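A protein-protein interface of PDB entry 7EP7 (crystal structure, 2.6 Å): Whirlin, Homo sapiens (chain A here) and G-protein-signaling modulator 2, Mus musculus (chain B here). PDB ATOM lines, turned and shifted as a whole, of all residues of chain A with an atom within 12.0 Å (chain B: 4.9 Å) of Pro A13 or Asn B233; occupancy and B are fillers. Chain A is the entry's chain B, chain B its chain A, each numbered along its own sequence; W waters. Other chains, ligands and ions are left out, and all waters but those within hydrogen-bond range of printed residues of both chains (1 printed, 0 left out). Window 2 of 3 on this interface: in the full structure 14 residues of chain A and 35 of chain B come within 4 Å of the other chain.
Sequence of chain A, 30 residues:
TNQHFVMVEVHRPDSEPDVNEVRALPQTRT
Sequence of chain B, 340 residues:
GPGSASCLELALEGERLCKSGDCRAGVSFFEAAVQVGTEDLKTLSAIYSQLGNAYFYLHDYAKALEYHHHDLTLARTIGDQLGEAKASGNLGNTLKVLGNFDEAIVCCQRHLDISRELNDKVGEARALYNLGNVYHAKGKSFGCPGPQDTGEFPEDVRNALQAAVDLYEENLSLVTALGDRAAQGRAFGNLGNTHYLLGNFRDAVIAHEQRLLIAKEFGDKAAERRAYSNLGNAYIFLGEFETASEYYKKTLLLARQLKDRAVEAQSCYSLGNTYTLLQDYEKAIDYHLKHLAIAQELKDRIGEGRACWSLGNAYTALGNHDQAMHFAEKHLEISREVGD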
ATOM      1  N   PRO A  13     -10.647   4.237 -31.035  1.00  0.00           N
ATOM      2  CA  PRO A  13      -9.230   4.302 -30.651  1.00  0.00           C
ATOM      3  C   PRO A  13      -8.310   4.580 -31.840  1.00  0.00           C
ATOM      4  O   PRO A  13      -8.227   3.738 -32.744  1.00  0.00           O
ATOM      5  CB  PRO A  13      -8.964   2.903 -30.071  1.00  0.00           C
ATOM      6  CG  PRO A  13     -10.326   2.478 -29.486  1.00  0.00           C
ATOM      7  CD  PRO A  13     -11.412   3.371 -30.119  1.00  0.00           C
ATOM      8  N   ASP A  14      -7.633   5.734 -31.830  1.00  0.00           N
ATOM      9  CA  ASP A  14      -6.789   6.170 -32.940  1.00  0.00           C
ATOM     10  C   ASP A  14      -5.332   6.088 -32.512  1.00  0.00           C
ATOM     11  O   ASP A  14      -4.911   6.814 -31.601  1.00  0.00           O
ATOM     12  CB  ASP A  14      -7.128   7.596 -33.368  1.00  0.00           C
ATOM     13  CG  ASP A  14      -8.406   7.678 -34.156  1.00  0.00           C
ATOM     14  OD1 ASP A  14      -8.411   7.238 -35.328  1.00  0.00           O
ATOM     15  OD2 ASP A  14      -9.410   8.173 -33.588  1.00  0.00           O
ATOM     16  N   SER A  15      -4.562   5.238 -33.191  1.00  0.00           N
ATOM     17  CA  SER A  15      -3.240   4.873 -32.711  1.00  0.00           C
ATOM     18  C   SER A  15      -2.213   5.891 -33.197  1.00  0.00           C
ATOM     19  O   SER A  15      -2.540   6.943 -33.745  1.00  0.00           O
ATOM     20  CB  SER A  15      -2.868   3.455 -33.159  1.00  0.00           C
ATOM     21  OG  SER A  15      -2.695   3.372 -34.570  1.00  0.00           O
ATOM     22  N   GLU A  16      -0.979   5.575 -33.000  1.00  0.00           N
ATOM     23  CA  GLU A  16       0.209   6.280 -33.380  1.00  0.00           C
ATOM     24  C   GLU A  16       0.899   5.551 -34.523  1.00  0.00           C
ATOM     25  O   GLU A  16       0.831   4.318 -34.619  1.00  0.00           O
ATOM     26  CB  GLU A  16       1.160   6.394 -32.181  1.00  0.00           C
ATOM     27  CG  GLU A  16       0.526   7.158 -31.035  1.00  0.00           C
ATOM     28  CD  GLU A  16       0.232   8.615 -31.396  1.00  0.00           C
ATOM     29  OE1 GLU A  16       1.116   9.295 -31.985  1.00  0.00           O
ATOM     30  OE2 GLU A  16      -0.918   9.050 -31.140  1.00  0.00           O
ATOM     31  N   PRO A  17       1.580   6.288 -35.393  1.00  0.00           N
ATOM     32  CA  PRO A  17       2.228   5.656 -36.544  1.00  0.00           C
ATOM     33  C   PRO A  17       3.374   4.736 -36.148  1.00  0.00           C
ATOM     34  O   PRO A  17       4.134   4.990 -35.207  1.00  0.00           O
ATOM     35  CB  PRO A  17       2.757   6.846 -37.356  1.00  0.00           C
ATOM     36  CG  PRO A  17       2.930   7.936 -36.319  1.00  0.00           C
ATOM     37  CD  PRO A  17       1.769   7.746 -35.385  1.00  0.00           C
ATOM     38  N   LYS B 140      -4.818  -6.269 -29.368  1.00  0.00           N
ATOM     39  CA  LYS B 140      -5.906  -5.595 -30.065  1.00  0.00           C
ATOM     40  C   LYS B 140      -6.588  -6.491 -31.102  1.00  0.00           C
ATOM     41  O   LYS B 140      -7.780  -6.319 -31.374  1.00  0.00           O
ATOM     42  CB  LYS B 140      -5.344  -4.339 -30.738  1.00  0.00           C
ATOM     43  CG  LYS B 140      -6.341  -3.310 -31.234  1.00  0.00           C
ATOM     44  CD  LYS B 140      -5.613  -2.179 -31.970  1.00  0.00           C
ATOM     45  CE  LYS B 140      -6.456  -0.904 -31.941  1.00  0.00           C
ATOM     46  NZ  LYS B 140      -6.480  -0.152 -33.235  1.00  0.00           N
ATOM     47  N   ASN B 193      -3.525   4.062 -25.317  1.00  0.00           N
ATOM     48  CA  ASN B 193      -4.513   3.172 -25.923  1.00  0.00           C
ATOM     49  C   ASN B 193      -4.393   1.749 -25.384  1.00  0.00           C
ATOM     50  O   ASN B 193      -5.404   1.033 -25.299  1.00  0.00           O
ATOM     51  CB  ASN B 193      -4.383   3.174 -27.436  1.00  0.00           C
ATOM     52  CG  ASN B 193      -4.965   4.417 -28.052  1.00  0.00           C
ATOM     53  OD1 ASN B 193      -5.829   5.074 -27.449  1.00  0.00           O
ATOM     54  ND2 ASN B 193      -4.518   4.745 -29.268  1.00  0.00           N
ATOM     55  N   TYR B 196      -6.071   1.701 -22.073  1.00  0.00           N
ATOM     56  CA  TYR B 196      -7.495   1.719 -22.369  1.00  0.00           C
ATOM     57  C   TYR B 196      -8.045   0.308 -22.531  1.00  0.00           C
ATOM     58  O   TYR B 196      -8.998  -0.092 -21.851  1.00  0.00           O
ATOM     59  CB  TYR B 196      -7.694   2.532 -23.635  1.00  0.00           C
ATOM     60  CG  TYR B 196      -9.106   2.655 -24.090  1.00  0.00           C
ATOM     61  CD1 TYR B 196     -10.013   3.472 -23.414  1.00  0.00           C
ATOM     62  CD2 TYR B 196      -9.534   1.966 -25.204  1.00  0.00           C
ATOM     63  CE1 TYR B 196     -11.316   3.594 -23.853  1.00  0.00           C
ATOM     64  CE2 TYR B 196     -10.808   2.078 -25.648  1.00  0.00           C
ATOM     65  CZ  TYR B 196     -11.703   2.888 -24.978  1.00  0.00           C
ATOM     66  OH  TYR B 196     -12.987   2.974 -25.462  1.00  0.00           O
ATOM     67  N   SER B 229     -10.306  12.813 -28.774  1.00  0.00           N
ATOM     68  CA  SER B 229     -11.124  11.632 -29.022  1.00  0.00           C
ATOM     69  C   SER B 229     -10.756  10.496 -28.078  1.00  0.00           C
ATOM     70  O   SER B 229     -11.614   9.950 -27.366  1.00  0.00           O
ATOM     71  CB  SER B 229     -10.954  11.183 -30.469  1.00  0.00           C
ATOM     72  OG  SER B 229     -11.378   9.838 -30.594  1.00  0.00           O
ATOM     73  N   ASN B 230      -9.485  10.092 -28.098  1.00  0.00           N
ATOM     74  CA  ASN B 230      -9.047   9.041 -27.193  1.00  0.00           C
ATOM     75  C   ASN B 230      -9.388   9.397 -25.753  1.00  0.00           C
ATOM     76  O   ASN B 230      -9.852   8.544 -24.984  1.00  0.00           O
ATOM     77  CB  ASN B 230      -7.555   8.803 -27.370  1.00  0.00           C
ATOM     78  CG  ASN B 230      -7.252   7.915 -28.542  1.00  0.00           C
ATOM     79  OD1 ASN B 230      -8.079   7.082 -28.946  1.00  0.00           O
ATOM     80  ND2 ASN B 230      -6.059   8.063 -29.095  1.00  0.00           N
ATOM     81  N   LEU B 231      -9.213  10.667 -25.379  1.00  0.00           N
ATOM     82  CA  LEU B 231      -9.648  11.102 -24.056  1.00  0.00           C
ATOM     83  C   LEU B 231     -11.151  10.941 -23.891  1.00  0.00           C
ATOM     84  O   LEU B 231     -11.625  10.559 -22.813  1.00  0.00           O
ATOM     85  CB  LEU B 231      -9.238  12.554 -23.810  1.00  0.00           C
ATOM     86  CG  LEU B 231      -7.811  12.676 -23.276  1.00  0.00           C
ATOM     87  CD1 LEU B 231      -7.214  14.023 -23.593  1.00  0.00           C
ATOM     88  CD2 LEU B 231      -7.787  12.378 -21.783  1.00  0.00           C
ATOM     89  N   GLY B 232     -11.919  11.242 -24.941  1.00  0.00           N
ATOM     90  CA  GLY B 232     -13.353  11.043 -24.864  1.00  0.00           C
ATOM     91  C   GLY B 232     -13.712   9.594 -24.601  1.00  0.00           C
ATOM     92  O   GLY B 232     -14.552   9.290 -23.741  1.00  0.00           O
ATOM     93  N   ASN B 233     -13.069   8.676 -25.334  1.00  0.00           N
ATOM     94  CA  ASN B 233     -13.304   7.253 -25.111  1.00  0.00           C
ATOM     95  C   ASN B 233     -13.148   6.912 -23.643  1.00  0.00           C
ATOM     96  O   ASN B 233     -14.022   6.275 -23.040  1.00  0.00           O
ATOM     97  CB  ASN B 233     -12.340   6.424 -25.954  1.00  0.00           C
ATOM     98  CG  ASN B 233     -12.545   6.626 -27.450  1.00  0.00           C
ATOM     99  OD1 ASN B 233     -13.506   7.273 -27.878  1.00  0.00           O
ATOM    100  ND2 ASN B 233     -11.618   6.101 -28.252  1.00  0.00           N
ATOM    101  N   ALA B 234     -12.049   7.372 -23.038  1.00  0.00           N
ATOM    102  CA  ALA B 234     -11.702   6.911 -21.701  1.00  0.00           C
ATOM    103  C   ALA B 234     -12.652   7.454 -20.637  1.00  0.00           C
ATOM    104  O   ALA B 234     -12.875   6.790 -19.616  1.00  0.00           O
ATOM    105  CB  ALA B 234     -10.259   7.287 -21.391  1.00  0.00           C
ATOM    106  N   TYR B 235     -13.230   8.639 -20.852  1.00  0.00           N
ATOM    107  CA  TYR B 235     -14.136   9.200 -19.850  1.00  0.00           C
ATOM    108  C   TYR B 235     -15.502   8.536 -19.901  1.00  0.00           C
ATOM    109  O   TYR B 235     -16.134   8.327 -18.856  1.00  0.00           O
ATOM    110  CB  TYR B 235     -14.264  10.708 -20.039  1.00  0.00           C
ATOM    111  CG  TYR B 235     -13.095  11.444 -19.456  1.00  0.00           C
ATOM    112  CD1 TYR B 235     -12.803  11.352 -18.101  1.00  0.00           C
ATOM    113  CD2 TYR B 235     -12.254  12.194 -20.265  1.00  0.00           C
ATOM    114  CE1 TYR B 235     -11.713  12.013 -17.556  1.00  0.00           C
ATOM    115  CE2 TYR B 235     -11.150  12.864 -19.732  1.00  0.00           C
ATOM    116  CZ  TYR B 235     -10.884  12.768 -18.376  1.00  0.00           C
ATOM    117  OH  TYR B 235      -9.792  13.425 -17.851  1.00  0.00           O
ATOM    118  N   ILE B 236     -15.970   8.201 -21.105  1.00  0.00           N
ATOM    119  CA  ILE B 236     -17.175   7.382 -21.234  1.00  0.00           C
ATOM    120  C   ILE B 236     -17.080   6.145 -20.344  1.00  0.00           C
ATOM    121  O   ILE B 236     -17.920   5.923 -19.461  1.00  0.00           O
ATOM    122  CB  ILE B 236     -17.410   6.994 -22.702  1.00  0.00           C
ATOM    123  CG1 ILE B 236     -17.968   8.189 -23.472  1.00  0.00           C
ATOM    124  CG2 ILE B 236     -18.333   5.799 -22.784  1.00  0.00           C
ATOM    125  CD1 ILE B 236     -19.282   8.692 -22.895  1.00  0.00           C
ATOM    126  N   PHE B 237     -16.045   5.322 -20.555  1.00  0.00           N
ATOM    127  CA  PHE B 237     -15.894   4.119 -19.740  1.00  0.00           C
ATOM    128  C   PHE B 237     -15.652   4.459 -18.278  1.00  0.00           C
ATOM    129  O   PHE B 237     -15.977   3.658 -17.390  1.00  0.00           O
ATOM    130  CB  PHE B 237     -14.757   3.263 -20.268  1.00  0.00           C
ATOM    131  CG  PHE B 237     -15.158   2.371 -21.392  1.00  0.00           C
ATOM    132  CD1 PHE B 237     -15.256   2.864 -22.673  1.00  0.00           C
ATOM    133  CD2 PHE B 237     -15.454   1.044 -21.163  1.00  0.00           C
ATOM    134  CE1 PHE B 237     -15.637   2.047 -23.716  1.00  0.00           C
ATOM    135  CE2 PHE B 237     -15.840   0.223 -22.196  1.00  0.00           C
ATOM    136  CZ  PHE B 237     -15.929   0.723 -23.479  1.00  0.00           C
ATOM    137  N   TYR B 248     -15.347  15.425 -26.778  1.00  0.00           N
ATOM    138  CA  TYR B 248     -15.785  15.036 -28.113  1.00  0.00           C
ATOM    139  C   TYR B 248     -16.026  16.264 -28.989  1.00  0.00           C
ATOM    140  O   TYR B 248     -15.607  16.299 -30.153  1.00  0.00           O
ATOM    141  CB  TYR B 248     -17.032  14.163 -28.002  1.00  0.00           C
ATOM    142  CG  TYR B 248     -16.721  12.718 -27.676  1.00  0.00           C
ATOM    143  CD1 TYR B 248     -17.473  12.016 -26.736  1.00  0.00           C
ATOM    144  CD2 TYR B 248     -15.671  12.051 -28.312  1.00  0.00           C
ATOM    145  CE1 TYR B 248     -17.187  10.680 -26.432  1.00  0.00           C
ATOM    146  CE2 TYR B 248     -15.375  10.726 -28.018  1.00  0.00           C
ATOM    147  CZ  TYR B 248     -16.143  10.044 -27.079  1.00  0.00           C
ATOM    148  OH  TYR B 248     -15.878   8.721 -26.788  1.00  0.00           O
HETATM  149  O   HOH W   1      -6.000   2.689 -33.349  1.00  0.00           O
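The side-chain amide nitrogen of Asn B193 is in hydrogen-bond range of the backbone carbonyl oxygen of Asp A14 (3.1 Å). ND2 of Asn B230 sits at hydrogen-bond distance from O of Asp A14 (3.0 Å). The backbone nitrogen (N) of Pro A13 sits close to the side-chain amide nitrogen (ND2) of Asn B233, 3.5 Å away.
Printed residues of chain B that touch a printed residue of chain A: Asn B193, Tyr B196, Ser B229, Asn B230 and Asn B233. Hydrophobic or aromatic side chains of chain B within 4 Å of the printed part of chain A: Tyr B196. Hydrophobic or aromatic side chains of chain A that line the printed part of chain B: Pro A13.
The side-chain amide oxygen (OD1) of Asn B230 sits close to the side-chain amide oxygen (OD1) of Asn B193, 3.4 Å away. O of Ser B229 lies close to OD1 of Asn B233 (3.3 Å). The side-chain amide oxygen (OD1) of Asn B233 sits at hydrogen-bond distance from the side-chain hydroxyl (OH) of Tyr B248 (3.0 Å).
Of chain B, only Tyr B196, Asn B230 and Asn B233 come within 4 Å of Pro A13. Asn B233 touches just one residue of chain A: Pro A13 (3.3 Å). Asn B193 touches two residues of chain A. Printed residues of chain A within 4 Å of Asn B230: Pro A13 and Asp A14. No residue of chain A comes within 4 Å of Ile B236. Printed residues of chain B within 4 Å of Ser A15: Asn B193 (3.7 Å). Of the printed residues of chain B, Asp A14 touches Asn B193, Ser B229 and Asn B230. Printed residues of chain A within 4 Å of Tyr B196: Pro A13 (3.9 Å). Tyr B235 touches none of the printed residues of chain A. The nearest residue of chain B that does not touch Pro A13 is Lys B140 (4.3 Å). The nearest residue of chain A that does not touch Asn B233 is Asp A14 (5.4 Å). The nearest printed residue of chain B that does not touch Ser A15 is Lys B140 (5.1 Å).
CE2 of Tyr B196 touches CG of Pro A13, at 3.9 Å. CA of Pro A13 touches OD1 of Asn B230 (3.5 Å). Ser B229 touches Asp A14 (OG to OD2, 3.95 Å). Ser A15 touches Asn B193 (CA to ND2, 3.7 Å).
Water W1 lies within hydrogen-bond range of the backbone carbonyl oxygen (O) of Pro A13 (2.5 Å), the side-chain amino group (NZ) of Lys B140 (2.9 Å) and the backbone NH (N) of Ser A15 (2.9 Å).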
